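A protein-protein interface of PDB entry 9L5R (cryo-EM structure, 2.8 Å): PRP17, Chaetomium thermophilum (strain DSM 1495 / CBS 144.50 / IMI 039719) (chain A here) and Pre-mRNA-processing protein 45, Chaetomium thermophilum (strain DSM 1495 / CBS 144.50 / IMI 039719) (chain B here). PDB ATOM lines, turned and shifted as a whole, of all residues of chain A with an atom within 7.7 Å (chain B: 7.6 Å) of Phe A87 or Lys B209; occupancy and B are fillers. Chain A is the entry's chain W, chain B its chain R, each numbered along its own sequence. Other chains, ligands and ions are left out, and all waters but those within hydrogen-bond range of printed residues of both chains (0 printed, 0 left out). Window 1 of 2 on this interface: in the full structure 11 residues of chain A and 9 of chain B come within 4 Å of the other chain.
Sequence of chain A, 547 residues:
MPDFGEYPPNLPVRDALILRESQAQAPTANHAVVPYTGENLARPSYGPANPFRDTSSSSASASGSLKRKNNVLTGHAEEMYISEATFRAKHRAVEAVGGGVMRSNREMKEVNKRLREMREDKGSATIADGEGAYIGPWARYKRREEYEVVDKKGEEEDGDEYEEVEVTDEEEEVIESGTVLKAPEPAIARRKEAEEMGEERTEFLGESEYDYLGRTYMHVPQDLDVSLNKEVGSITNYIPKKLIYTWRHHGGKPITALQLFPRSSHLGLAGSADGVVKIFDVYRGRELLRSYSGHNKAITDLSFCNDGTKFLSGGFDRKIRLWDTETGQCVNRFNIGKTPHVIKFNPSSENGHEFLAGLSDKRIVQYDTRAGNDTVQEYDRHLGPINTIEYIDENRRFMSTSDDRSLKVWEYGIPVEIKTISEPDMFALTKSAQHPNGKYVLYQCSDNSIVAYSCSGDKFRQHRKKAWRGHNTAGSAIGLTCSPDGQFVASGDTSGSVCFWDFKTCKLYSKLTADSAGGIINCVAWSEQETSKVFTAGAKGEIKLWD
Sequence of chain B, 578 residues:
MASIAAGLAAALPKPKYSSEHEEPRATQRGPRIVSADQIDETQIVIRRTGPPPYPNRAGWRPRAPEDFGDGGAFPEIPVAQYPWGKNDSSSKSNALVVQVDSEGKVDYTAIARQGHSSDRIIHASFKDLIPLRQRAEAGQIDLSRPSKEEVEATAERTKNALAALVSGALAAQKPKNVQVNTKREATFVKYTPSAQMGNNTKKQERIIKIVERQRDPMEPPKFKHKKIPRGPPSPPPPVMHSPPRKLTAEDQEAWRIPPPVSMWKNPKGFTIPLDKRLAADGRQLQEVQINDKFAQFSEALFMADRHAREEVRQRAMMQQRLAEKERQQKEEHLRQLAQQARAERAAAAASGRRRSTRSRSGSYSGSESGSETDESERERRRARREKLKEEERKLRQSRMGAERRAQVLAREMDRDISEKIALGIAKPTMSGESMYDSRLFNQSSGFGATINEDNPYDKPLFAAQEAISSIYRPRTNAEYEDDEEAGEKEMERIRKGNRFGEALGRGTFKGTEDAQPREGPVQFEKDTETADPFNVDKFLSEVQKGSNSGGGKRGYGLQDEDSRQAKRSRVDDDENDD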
ATOM      1  N   MET A  80     -10.107 -25.927  15.043  1.00  0.00           N
ATOM      2  CA  MET A  80      -8.771 -25.782  15.589  1.00  0.00           C
ATOM      3  C   MET A  80      -8.491 -26.961  16.510  1.00  0.00           C
ATOM      4  O   MET A  80      -9.404 -27.649  16.968  1.00  0.00           O
ATOM      5  CB  MET A  80      -8.651 -24.446  16.325  1.00  0.00           C
ATOM      6  CG  MET A  80      -7.271 -24.036  16.741  1.00  0.00           C
ATOM      7  SD  MET A  80      -7.442 -22.506  17.609  1.00  0.00           S
ATOM      8  CE  MET A  80      -8.332 -23.202  18.965  1.00  0.00           C
ATOM      9  N   ILE A  82      -6.035 -27.107  19.382  1.00  0.00           N
ATOM     10  CA  ILE A  82      -5.149 -26.843  20.509  1.00  0.00           C
ATOM     11  C   ILE A  82      -5.341 -27.908  21.573  1.00  0.00           C
ATOM     12  O   ILE A  82      -6.258 -28.731  21.498  1.00  0.00           O
ATOM     13  CB  ILE A  82      -5.362 -25.451  21.120  1.00  0.00           C
ATOM     14  CG1 ILE A  82      -6.769 -25.325  21.694  1.00  0.00           C
ATOM     15  CG2 ILE A  82      -5.055 -24.374  20.098  1.00  0.00           C
ATOM     16  CD1 ILE A  82      -6.834 -24.388  22.861  1.00  0.00           C
ATOM     17  N   SER A  83      -4.462 -27.901  22.562  1.00  0.00           N
ATOM     18  CA  SER A  83      -4.468 -28.869  23.642  1.00  0.00           C
ATOM     19  C   SER A  83      -5.396 -28.437  24.770  1.00  0.00           C
ATOM     20  O   SER A  83      -5.624 -27.243  25.008  1.00  0.00           O
ATOM     21  CB  SER A  83      -3.054 -29.065  24.175  1.00  0.00           C
ATOM     22  OG  SER A  83      -3.047 -29.907  25.305  1.00  0.00           O
ATOM     23  N   GLU A  84      -5.932 -29.440  25.465  1.00  0.00           N
ATOM     24  CA  GLU A  84      -6.861 -29.191  26.557  1.00  0.00           C
ATOM     25  C   GLU A  84      -6.184 -28.449  27.697  1.00  0.00           C
ATOM     26  O   GLU A  84      -6.782 -27.562  28.313  1.00  0.00           O
ATOM     27  CB  GLU A  84      -7.451 -30.514  27.037  1.00  0.00           C
ATOM     28  CG  GLU A  84      -8.558 -30.361  28.051  1.00  0.00           C
ATOM     29  CD  GLU A  84      -9.844 -29.858  27.439  1.00  0.00           C
ATOM     30  OE1 GLU A  84     -10.224 -30.361  26.363  1.00  0.00           O
ATOM     31  OE2 GLU A  84     -10.470 -28.960  28.032  1.00  0.00           O
ATOM     32  N   ALA A  85      -4.929 -28.798  27.983  1.00  0.00           N
ATOM     33  CA  ALA A  85      -4.168 -28.099  29.010  1.00  0.00           C
ATOM     34  C   ALA A  85      -3.925 -26.649  28.627  1.00  0.00           C
ATOM     35  O   ALA A  85      -3.968 -25.761  29.485  1.00  0.00           O
ATOM     36  CB  ALA A  85      -2.845 -28.815  29.250  1.00  0.00           C
ATOM     37  N   THR A  86      -3.659 -26.397  27.342  1.00  0.00           N
ATOM     38  CA  THR A  86      -3.493 -25.033  26.850  1.00  0.00           C
ATOM     39  C   THR A  86      -4.745 -24.210  27.088  1.00  0.00           C
ATOM     40  O   THR A  86      -4.676 -23.098  27.635  1.00  0.00           O
ATOM     41  CB  THR A  86      -3.159 -25.047  25.358  1.00  0.00           C
ATOM     42  OG1 THR A  86      -1.948 -25.772  25.133  1.00  0.00           O
ATOM     43  CG2 THR A  86      -2.998 -23.640  24.840  1.00  0.00           C
ATOM     44  N   PHE A  87      -5.904 -24.755  26.700  1.00  0.00           N
ATOM     45  CA  PHE A  87      -7.155 -24.032  26.905  1.00  0.00           C
ATOM     46  C   PHE A  87      -7.426 -23.794  28.381  1.00  0.00           C
ATOM     47  O   PHE A  87      -7.838 -22.697  28.767  1.00  0.00           O
ATOM     48  CB  PHE A  87      -8.335 -24.773  26.278  1.00  0.00           C
ATOM     49  CG  PHE A  87      -9.634 -24.018  26.384  1.00  0.00           C
ATOM     50  CD1 PHE A  87      -9.994 -23.110  25.410  1.00  0.00           C
ATOM     51  CD2 PHE A  87     -10.485 -24.200  27.465  1.00  0.00           C
ATOM     52  CE1 PHE A  87     -11.162 -22.407  25.516  1.00  0.00           C
ATOM     53  CE2 PHE A  87     -11.641 -23.487  27.572  1.00  0.00           C
ATOM     54  CZ  PHE A  87     -11.985 -22.598  26.598  1.00  0.00           C
ATOM     55  N   ARG A  88      -7.219 -24.814  29.215  1.00  0.00           N
ATOM     56  CA  ARG A  88      -7.531 -24.678  30.631  1.00  0.00           C
ATOM     57  C   ARG A  88      -6.618 -23.667  31.304  1.00  0.00           C
ATOM     58  O   ARG A  88      -7.071 -22.878  32.138  1.00  0.00           O
ATOM     59  CB  ARG A  88      -7.434 -26.035  31.316  1.00  0.00           C
ATOM     60  CG  ARG A  88      -8.696 -26.860  31.222  1.00  0.00           C
ATOM     61  CD  ARG A  88      -8.412 -28.295  31.578  1.00  0.00           C
ATOM     62  NE  ARG A  88      -9.544 -29.171  31.319  1.00  0.00           N
ATOM     63  CZ  ARG A  88     -10.416 -29.553  32.239  1.00  0.00           C
ATOM     64  NH1 ARG A  88     -10.326 -29.135  33.490  1.00  0.00           N
ATOM     65  NH2 ARG A  88     -11.405 -30.370  31.893  1.00  0.00           N
ATOM     66  N   ALA A  89      -5.344 -23.639  30.917  1.00  0.00           N
ATOM     67  CA  ALA A  89      -4.408 -22.702  31.518  1.00  0.00           C
ATOM     68  C   ALA A  89      -4.709 -21.269  31.104  1.00  0.00           C
ATOM     69  O   ALA A  89      -4.685 -20.364  31.943  1.00  0.00           O
ATOM     70  CB  ALA A  89      -2.980 -23.080  31.145  1.00  0.00           C
ATOM     71  N   LYS A  90      -4.988 -21.039  29.818  1.00  0.00           N
ATOM     72  CA  LYS A  90      -5.301 -19.680  29.383  1.00  0.00           C
ATOM     73  C   LYS A  90      -6.618 -19.196  29.980  1.00  0.00           C
ATOM     74  O   LYS A  90      -6.733 -18.034  30.404  1.00  0.00           O
ATOM     75  CB  LYS A  90      -5.334 -19.625  27.863  1.00  0.00           C
ATOM     76  CG  LYS A  90      -3.967 -19.794  27.260  1.00  0.00           C
ATOM     77  CD  LYS A  90      -3.984 -19.668  25.762  1.00  0.00           C
ATOM     78  CE  LYS A  90      -2.592 -19.861  25.199  1.00  0.00           C
ATOM     79  NZ  LYS A  90      -1.613 -18.916  25.787  1.00  0.00           N
ATOM     80  N   HIS A  91      -7.610 -20.087  30.047  1.00  0.00           N
ATOM     81  CA  HIS A  91      -8.879 -19.755  30.672  1.00  0.00           C
ATOM     82  C   HIS A  91      -8.697 -19.416  32.141  1.00  0.00           C
ATOM     83  O   HIS A  91      -9.311 -18.473  32.641  1.00  0.00           O
ATOM     84  CB  HIS A  91      -9.849 -20.920  30.506  1.00  0.00           C
ATOM     85  CG  HIS A  91     -11.269 -20.569  30.797  1.00  0.00           C
ATOM     86  ND1 HIS A  91     -11.739 -20.355  32.073  1.00  0.00           N
ATOM     87  CD2 HIS A  91     -12.324 -20.398  29.973  1.00  0.00           C
ATOM     88  CE1 HIS A  91     -13.024 -20.063  32.019  1.00  0.00           C
ATOM     89  NE2 HIS A  91     -13.403 -20.081  30.757  1.00  0.00           N
ATOM     90  N   ARG A  92      -7.847 -20.166  32.840  1.00  0.00           N
ATOM     91  CA  ARG A  92      -7.547 -19.873  34.236  1.00  0.00           C
ATOM     92  C   ARG A  92      -6.841 -18.545  34.402  1.00  0.00           C
ATOM     93  O   ARG A  92      -7.102 -17.816  35.365  1.00  0.00           O
ATOM     94  CB  ARG A  92      -6.698 -20.988  34.816  1.00  0.00           C
ATOM     95  CG  ARG A  92      -6.353 -20.820  36.265  1.00  0.00           C
ATOM     96  CD  ARG A  92      -7.602 -20.876  37.055  1.00  0.00           C
ATOM     97  NE  ARG A  92      -8.243 -22.149  36.799  1.00  0.00           N
ATOM     98  CZ  ARG A  92      -7.955 -23.280  37.411  1.00  0.00           C
ATOM     99  NH1 ARG A  92      -6.998 -23.354  38.317  1.00  0.00           N
ATOM    100  NH2 ARG A  92      -8.633 -24.372  37.084  1.00  0.00           N
ATOM    101  N   ALA A  93      -5.918 -18.235  33.492  1.00  0.00           N
ATOM    102  CA  ALA A  93      -5.185 -16.981  33.578  1.00  0.00           C
ATOM    103  C   ALA A  93      -6.127 -15.799  33.456  1.00  0.00           C
ATOM    104  O   ALA A  93      -5.970 -14.796  34.158  1.00  0.00           O
ATOM    105  CB  ALA A  93      -4.113 -16.927  32.497  1.00  0.00           C
ATOM    106  N   GLU B 185     -16.030 -35.762  23.728  1.00  0.00           N
ATOM    107  CA  GLU B 185     -14.893 -34.855  23.657  1.00  0.00           C
ATOM    108  C   GLU B 185     -15.330 -33.481  23.158  1.00  0.00           C
ATOM    109  O   GLU B 185     -16.448 -33.283  22.680  1.00  0.00           O
ATOM    110  CB  GLU B 185     -13.794 -35.417  22.754  1.00  0.00           C
ATOM    111  CG  GLU B 185     -14.152 -35.462  21.272  1.00  0.00           C
ATOM    112  CD  GLU B 185     -14.921 -36.714  20.877  1.00  0.00           C
ATOM    113  OE1 GLU B 185     -15.438 -37.410  21.766  1.00  0.00           O
ATOM    114  OE2 GLU B 185     -15.008 -37.008  19.669  1.00  0.00           O
ATOM    115  N   ALA B 186     -14.421 -32.523  23.278  1.00  0.00           N
ATOM    116  CA  ALA B 186     -14.687 -31.133  22.963  1.00  0.00           C
ATOM    117  C   ALA B 186     -14.117 -30.767  21.602  1.00  0.00           C
ATOM    118  O   ALA B 186     -13.065 -31.258  21.191  1.00  0.00           O
ATOM    119  CB  ALA B 186     -14.087 -30.215  24.023  1.00  0.00           C
ATOM    120  N   THR B 187     -14.833 -29.896  20.903  1.00  0.00           N
ATOM    121  CA  THR B 187     -14.346 -29.257  19.695  1.00  0.00           C
ATOM    122  C   THR B 187     -13.797 -27.889  20.073  1.00  0.00           C
ATOM    123  O   THR B 187     -14.316 -27.235  20.979  1.00  0.00           O
ATOM    124  CB  THR B 187     -15.478 -29.130  18.673  1.00  0.00           C
ATOM    125  OG1 THR B 187     -15.970 -30.432  18.351  1.00  0.00           O
ATOM    126  CG2 THR B 187     -15.021 -28.461  17.394  1.00  0.00           C
ATOM    127  N   PHE B 188     -12.723 -27.473  19.415  1.00  0.00           N
ATOM    128  CA  PHE B 188     -12.199 -26.129  19.576  1.00  0.00           C
ATOM    129  C   PHE B 188     -12.377 -25.357  18.277  1.00  0.00           C
ATOM    130  O   PHE B 188     -12.203 -25.909  17.188  1.00  0.00           O
ATOM    131  CB  PHE B 188     -10.734 -26.163  19.999  1.00  0.00           C
ATOM    132  CG  PHE B 188     -10.530 -26.621  21.411  1.00  0.00           C
ATOM    133  CD1 PHE B 188     -10.794 -25.776  22.469  1.00  0.00           C
ATOM    134  CD2 PHE B 188     -10.089 -27.902  21.682  1.00  0.00           C
ATOM    135  CE1 PHE B 188     -10.617 -26.193  23.762  1.00  0.00           C
ATOM    136  CE2 PHE B 188      -9.908 -28.318  22.978  1.00  0.00           C
ATOM    137  CZ  PHE B 188     -10.170 -27.460  24.017  1.00  0.00           C
ATOM    138  N   VAL B 189     -12.763 -24.094  18.397  1.00  0.00           N
ATOM    139  CA  VAL B 189     -13.034 -23.228  17.254  1.00  0.00           C
ATOM    140  C   VAL B 189     -12.217 -21.958  17.435  1.00  0.00           C
ATOM    141  O   VAL B 189     -12.164 -21.396  18.530  1.00  0.00           O
ATOM    142  CB  VAL B 189     -14.545 -22.928  17.115  1.00  0.00           C
ATOM    143  CG1 VAL B 189     -14.801 -21.775  16.183  1.00  0.00           C
ATOM    144  CG2 VAL B 189     -15.283 -24.150  16.614  1.00  0.00           C
ATOM    145  N   ARG B 206     -10.789 -15.277  19.421  1.00  0.00           N
ATOM    146  CA  ARG B 206     -11.536 -16.059  20.403  1.00  0.00           C
ATOM    147  C   ARG B 206     -11.433 -17.558  20.160  1.00  0.00           C
ATOM    148  O   ARG B 206     -11.772 -18.052  19.071  1.00  0.00           O
ATOM    149  CB  ARG B 206     -13.003 -15.640  20.416  1.00  0.00           C
ATOM    150  CG  ARG B 206     -13.304 -14.537  21.379  1.00  0.00           C
ATOM    151  CD  ARG B 206     -14.756 -14.532  21.723  1.00  0.00           C
ATOM    152  NE  ARG B 206     -15.176 -13.251  22.266  1.00  0.00           N
ATOM    153  CZ  ARG B 206     -15.430 -13.045  23.547  1.00  0.00           C
ATOM    154  NH1 ARG B 206     -15.279 -14.001  24.440  1.00  0.00           N
ATOM    155  NH2 ARG B 206     -15.849 -11.849  23.943  1.00  0.00           N
ATOM    156  N   ILE B 207     -11.043 -18.273  21.215  1.00  0.00           N
ATOM    157  CA  ILE B 207     -10.987 -19.731  21.251  1.00  0.00           C
ATOM    158  C   ILE B 207     -12.246 -20.251  21.936  1.00  0.00           C
ATOM    159  O   ILE B 207     -12.508 -19.930  23.097  1.00  0.00           O
ATOM    160  CB  ILE B 207      -9.736 -20.210  21.999  1.00  0.00           C
ATOM    161  CG1 ILE B 207      -8.486 -19.454  21.540  1.00  0.00           C
ATOM    162  CG2 ILE B 207      -9.604 -21.703  21.904  1.00  0.00           C
ATOM    163  CD1 ILE B 207      -8.062 -19.730  20.134  1.00  0.00           C
ATOM    164  N   ILE B 208     -13.016 -21.072  21.231  1.00  0.00           N
ATOM    165  CA  ILE B 208     -14.300 -21.563  21.709  1.00  0.00           C
ATOM    166  C   ILE B 208     -14.155 -23.051  21.991  1.00  0.00           C
ATOM    167  O   ILE B 208     -13.709 -23.806  21.121  1.00  0.00           O
ATOM    168  CB  ILE B 208     -15.417 -21.331  20.680  1.00  0.00           C
ATOM    169  CG1 ILE B 208     -15.377 -19.916  20.096  1.00  0.00           C
ATOM    170  CG2 ILE B 208     -16.757 -21.530  21.341  1.00  0.00           C
ATOM    171  CD1 ILE B 208     -15.599 -18.821  21.063  1.00  0.00           C
ATOM    172  N   LYS B 209     -14.533 -23.471  23.195  1.00  0.00           N
ATOM    173  CA  LYS B 209     -14.597 -24.881  23.561  1.00  0.00           C
ATOM    174  C   LYS B 209     -16.057 -25.310  23.560  1.00  0.00           C
ATOM    175  O   LYS B 209     -16.821 -24.922  24.444  1.00  0.00           O
ATOM    176  CB  LYS B 209     -13.973 -25.119  24.931  1.00  0.00           C
ATOM    177  CG  LYS B 209     -13.904 -26.573  25.316  1.00  0.00           C
ATOM    178  CD  LYS B 209     -13.048 -26.774  26.526  1.00  0.00           C
ATOM    179  CE  LYS B 209     -13.545 -27.927  27.362  1.00  0.00           C
ATOM    180  NZ  LYS B 209     -12.920 -27.899  28.701  1.00  0.00           N
ATOM    181  N   ILE B 210     -16.441 -26.125  22.588  1.00  0.00           N
ATOM    182  CA  ILE B 210     -17.821 -26.554  22.425  1.00  0.00           C
ATOM    183  C   ILE B 210     -17.911 -28.019  22.813  1.00  0.00           C
ATOM    184  O   ILE B 210     -17.228 -28.866  22.229  1.00  0.00           O
ATOM    185  CB  ILE B 210     -18.318 -26.342  20.988  1.00  0.00           C
ATOM    186  CG1 ILE B 210     -18.052 -24.907  20.536  1.00  0.00           C
ATOM    187  CG2 ILE B 210     -19.787 -26.670  20.888  1.00  0.00           C
ATOM    188  CD1 ILE B 210     -18.523 -24.610  19.145  1.00  0.00           C
ATOM    189  N   VAL B 211     -18.758 -28.320  23.794  1.00  0.00           N
ATOM    190  CA  VAL B 211     -19.066 -29.692  24.169  1.00  0.00           C
ATOM    191  C   VAL B 211     -20.558 -29.928  23.975  1.00  0.00           C
ATOM    192  O   VAL B 211     -21.375 -29.014  24.098  1.00  0.00           O
ATOM    193  CB  VAL B 211     -18.627 -30.016  25.619  1.00  0.00           C
ATOM    194  CG1 VAL B 211     -17.210 -29.591  25.836  1.00  0.00           C
ATOM    195  CG2 VAL B 211     -19.501 -29.324  26.631  1.00  0.00           C
ATOM    196  N   GLU B 212     -20.901 -31.153  23.598  1.00  0.00           N
ATOM    197  CA  GLU B 212     -22.294 -31.568  23.543  1.00  0.00           C
ATOM    198  C   GLU B 212     -22.824 -31.764  24.957  1.00  0.00           C
ATOM    199  O   GLU B 212     -22.159 -32.351  25.805  1.00  0.00           O
ATOM    200  CB  GLU B 212     -22.419 -32.854  22.729  1.00  0.00           C
ATOM    201  CG  GLU B 212     -23.831 -33.301  22.433  1.00  0.00           C
ATOM    202  CD  GLU B 212     -23.896 -34.735  21.933  1.00  0.00           C
ATOM    203  OE1 GLU B 212     -23.246 -35.042  20.915  1.00  0.00           O
ATOM    204  OE2 GLU B 212     -24.587 -35.567  22.558  1.00  0.00           O
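OE2 of Glu A84 lies within salt-bridge range of NZ of Lys B209, 2.8 Å away.
The backbone carbonyl oxygen (O) of Phe B188 sits at hydrogen-bond distance from the backbone NH (N) of Met A80.
OE2 of Glu A84 is in salt-bridge range of NE of Arg A88, 3.4 Å away.
Among the printed residues, merely in contact across the chains: Met A80 with Ile B207 (3.5 Å), Ile A82 with Phe B188 (3.9 Å), Ile A82 with Ile B207 (3.97 Å), Glu A84 with Phe B188 (3.7 Å), Phe A87 with Phe B188 (3.5 Å), Phe A87 with Ile B207 (3.7 Å) and Phe A87 with Lys B209 (3.6 Å).
Phe A87 touches three residues of chain B.
Lys B209 touches two residues of chain A.
Of the printed residues of chain A, Ile B207 touches Met A80, Ile A82 and Phe A87.
Of the printed residues of chain B, Met A80 touches Phe B188 (3.0 Å) and Ile B207 (3.5 Å).
Arg A92 touches none of the printed residues of chain B.
The nearest residue of chain A that does not touch Lys B209 is Arg A88 (4.3 Å).
The nearest printed residue of chain B that does not touch Met A80 is Val B189 (4.3 Å).
Printed residues of chain B that touch a printed residue of chain A: Phe B188, Ile B207 and Lys B209.
Hydrophobic or aromatic side chains of chain B within 4 Å of the printed part of chain A: Phe B188 and Ile B207.
Of the 13 printed residues of chain A, 4 touch a printed residue of chain B.
Hydrophobic or aromatic side chains of chain A within 4 Å of the printed part of chain B: Met A80, Ile A82 and Phe A87.
Among the printed residues, 9 pairs touch across the chains.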
